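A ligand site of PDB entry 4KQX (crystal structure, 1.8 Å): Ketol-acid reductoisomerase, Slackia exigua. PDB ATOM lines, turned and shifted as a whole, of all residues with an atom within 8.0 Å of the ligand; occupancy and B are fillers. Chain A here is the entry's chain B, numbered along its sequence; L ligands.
O of Glu 344 sits at hydrogen-bond distance from N1 of the ligand (2.7 Å).
A nitrogen (N1) of the ligand lies close to the backbone NH of Glu 344, at 2.7 Å.
O of Leu 343 sits close to N2 of the ligand, 3.2 Å away.
N1 of the ligand lies within hydrogen-bond range of O of Glu 341 (3.5 Å).
O of Asp 342 sits at hydrogen-bond distance from N1 of the ligand, 2.8 Å away.
Within 4 Å of the ligand: Glu 341, Asp 342, Leu 343 and Glu 344.
The nearest printed residue that does not touch the ligand is Lys 340 (5.9 Å).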
ATOM      1  N   ILE A 338      -3.529   7.556  10.419  1.00  0.00           N
ATOM      2  CA  ILE A 338      -3.884   6.200   9.966  1.00  0.00           C
ATOM      3  C   ILE A 338      -2.752   5.193  10.245  1.00  0.00           C
ATOM      4  O   ILE A 338      -3.021   4.149  10.787  1.00  0.00           O
ATOM      5  CB  ILE A 338      -4.324   6.121   8.472  1.00  0.00           C
ATOM      6  CG1 ILE A 338      -5.756   6.700   8.295  1.00  0.00           C
ATOM      7  CG2 ILE A 338      -4.283   4.689   7.974  1.00  0.00           C
ATOM      8  CD1 ILE A 338      -6.485   6.363   6.990  1.00  0.00           C
ATOM      9  N   LYS A 339      -1.493   5.507   9.888  1.00  0.00           N
ATOM     10  CA  LYS A 339      -0.329   4.598  10.245  1.00  0.00           C
ATOM     11  C   LYS A 339      -0.144   4.480  11.740  1.00  0.00           C
ATOM     12  O   LYS A 339       0.216   3.380  12.279  1.00  0.00           O
ATOM     13  CB  LYS A 339       0.990   5.056   9.622  1.00  0.00           C
ATOM     14  CG  LYS A 339       0.945   5.078   8.104  1.00  0.00           C
ATOM     15  CD  LYS A 339       2.265   4.635   7.507  1.00  0.00           C
ATOM     16  CE  LYS A 339       2.318   5.047   6.026  1.00  0.00           C
ATOM     17  NZ  LYS A 339       1.412   4.235   5.166  1.00  0.00           N
ATOM     18  N   LYS A 340      -0.379   5.620  12.434  1.00  0.00           N
ATOM     19  CA  LYS A 340      -0.304   5.626  13.910  1.00  0.00           C
ATOM     20  C   LYS A 340      -1.397   4.702  14.437  1.00  0.00           C
ATOM     21  O   LYS A 340      -1.124   3.800  15.227  1.00  0.00           O
ATOM     22  CB  LYS A 340      -0.398   7.060  14.513  1.00  0.00           C
ATOM     23  CG  LYS A 340       0.947   7.787  14.629  1.00  0.00           C
ATOM     24  CD  LYS A 340       1.961   6.905  15.379  1.00  0.00           C
ATOM     25  CE  LYS A 340       3.375   7.489  15.474  1.00  0.00           C
ATOM     26  NZ  LYS A 340       4.366   6.376  15.700  1.00  0.00           N
ATOM     27  N   GLU A 341      -2.622   4.911  13.973  1.00  0.00           N
ATOM     28  CA  GLU A 341      -3.737   4.071  14.394  1.00  0.00           C
ATOM     29  C   GLU A 341      -3.543   2.582  14.014  1.00  0.00           C
ATOM     30  O   GLU A 341      -3.840   1.707  14.813  1.00  0.00           O
ATOM     31  CB  GLU A 341      -5.038   4.606  13.803  1.00  0.00           C
ATOM     32  CG  GLU A 341      -6.241   3.856  14.331  1.00  0.00           C
ATOM     33  CD  GLU A 341      -7.517   4.322  13.667  1.00  0.00           C
ATOM     34  OE1 GLU A 341      -7.733   3.944  12.475  1.00  0.00           O
ATOM     35  OE2 GLU A 341      -8.302   5.061  14.322  1.00  0.00           O
ATOM     36  N   ASP A 342      -3.036   2.306  12.800  1.00  0.00           N
ATOM     37  CA  ASP A 342      -2.769   0.894  12.365  1.00  0.00           C
ATOM     38  C   ASP A 342      -1.856   0.196  13.361  1.00  0.00           C
ATOM     39  O   ASP A 342      -2.057  -0.974  13.661  1.00  0.00           O
ATOM     40  CB  ASP A 342      -2.105   0.825  10.975  1.00  0.00           C
ATOM     41  CG  ASP A 342      -3.078   1.191   9.828  1.00  0.00           C
ATOM     42  OD1 ASP A 342      -4.320   0.993  10.002  1.00  0.00           O
ATOM     43  OD2 ASP A 342      -2.595   1.650   8.773  1.00  0.00           O
ATOM     44  N   LEU A 343      -0.855   0.929  13.846  1.00  0.00           N
ATOM     45  CA  LEU A 343       0.103   0.430  14.836  1.00  0.00           C
ATOM     46  C   LEU A 343      -0.570   0.013  16.138  1.00  0.00           C
ATOM     47  O   LEU A 343       0.022  -0.768  16.930  1.00  0.00           O
ATOM     48  CB  LEU A 343       1.148   1.535  15.187  1.00  0.00           C
ATOM     49  CG  LEU A 343       2.256   1.677  14.154  1.00  0.00           C
ATOM     50  CD1 LEU A 343       3.272   2.730  14.570  1.00  0.00           C
ATOM     51  CD2 LEU A 343       2.897   0.310  13.927  1.00  0.00           C
ATOM     52  N   GLU A 344      -1.770   0.562  16.371  1.00  0.00           N
ATOM     53  CA  GLU A 344      -2.309   0.551  17.732  1.00  0.00           C
ATOM     54  C   GLU A 344      -2.252  -0.725  18.601  1.00  0.00           C
ATOM     55  O   GLU A 344      -1.876  -1.825  18.150  1.00  0.00           O
ATOM     56  CB  GLU A 344      -3.596   1.369  17.918  1.00  0.00           C
ATOM     57  CG  GLU A 344      -3.245   2.621  18.733  1.00  0.00           C
ATOM     58  CD  GLU A 344      -2.199   2.331  19.825  1.00  0.00           C
ATOM     59  OE1 GLU A 344      -2.579   1.925  20.940  1.00  0.00           O
ATOM     60  OE2 GLU A 344      -0.972   2.478  19.593  1.00  0.00           O
HETATM   61  N1  LIG L   1      -3.490  -1.513  16.051  1.00  0.00           N
HETATM   62  C1  LIG L   1      -4.083  -2.824  15.673  1.00  0.00           C
HETATM   63  C2  LIG L   1      -5.488  -2.897  16.189  1.00  0.00           C
HETATM   64  O1  LIG L   1      -6.132  -1.833  16.271  1.00  0.00           O
HETATM   65  C3  LIG L   1      -3.195  -3.987  16.132  1.00  0.00           C
HETATM   66  C4  LIG L   1      -1.949  -4.109  15.290  1.00  0.00           C
HETATM   67  N2  LIG L   1      -0.771  -3.544  15.650  1.00  0.00           N
HETATM   68  C5  LIG L   1      -1.757  -4.659  14.009  1.00  0.00           C
HETATM   69  C6  LIG L   1       0.139  -3.756  14.673  1.00  0.00           C
HETATM   70  N3  LIG L   1      -0.465  -4.437  13.663  1.00  0.00           N
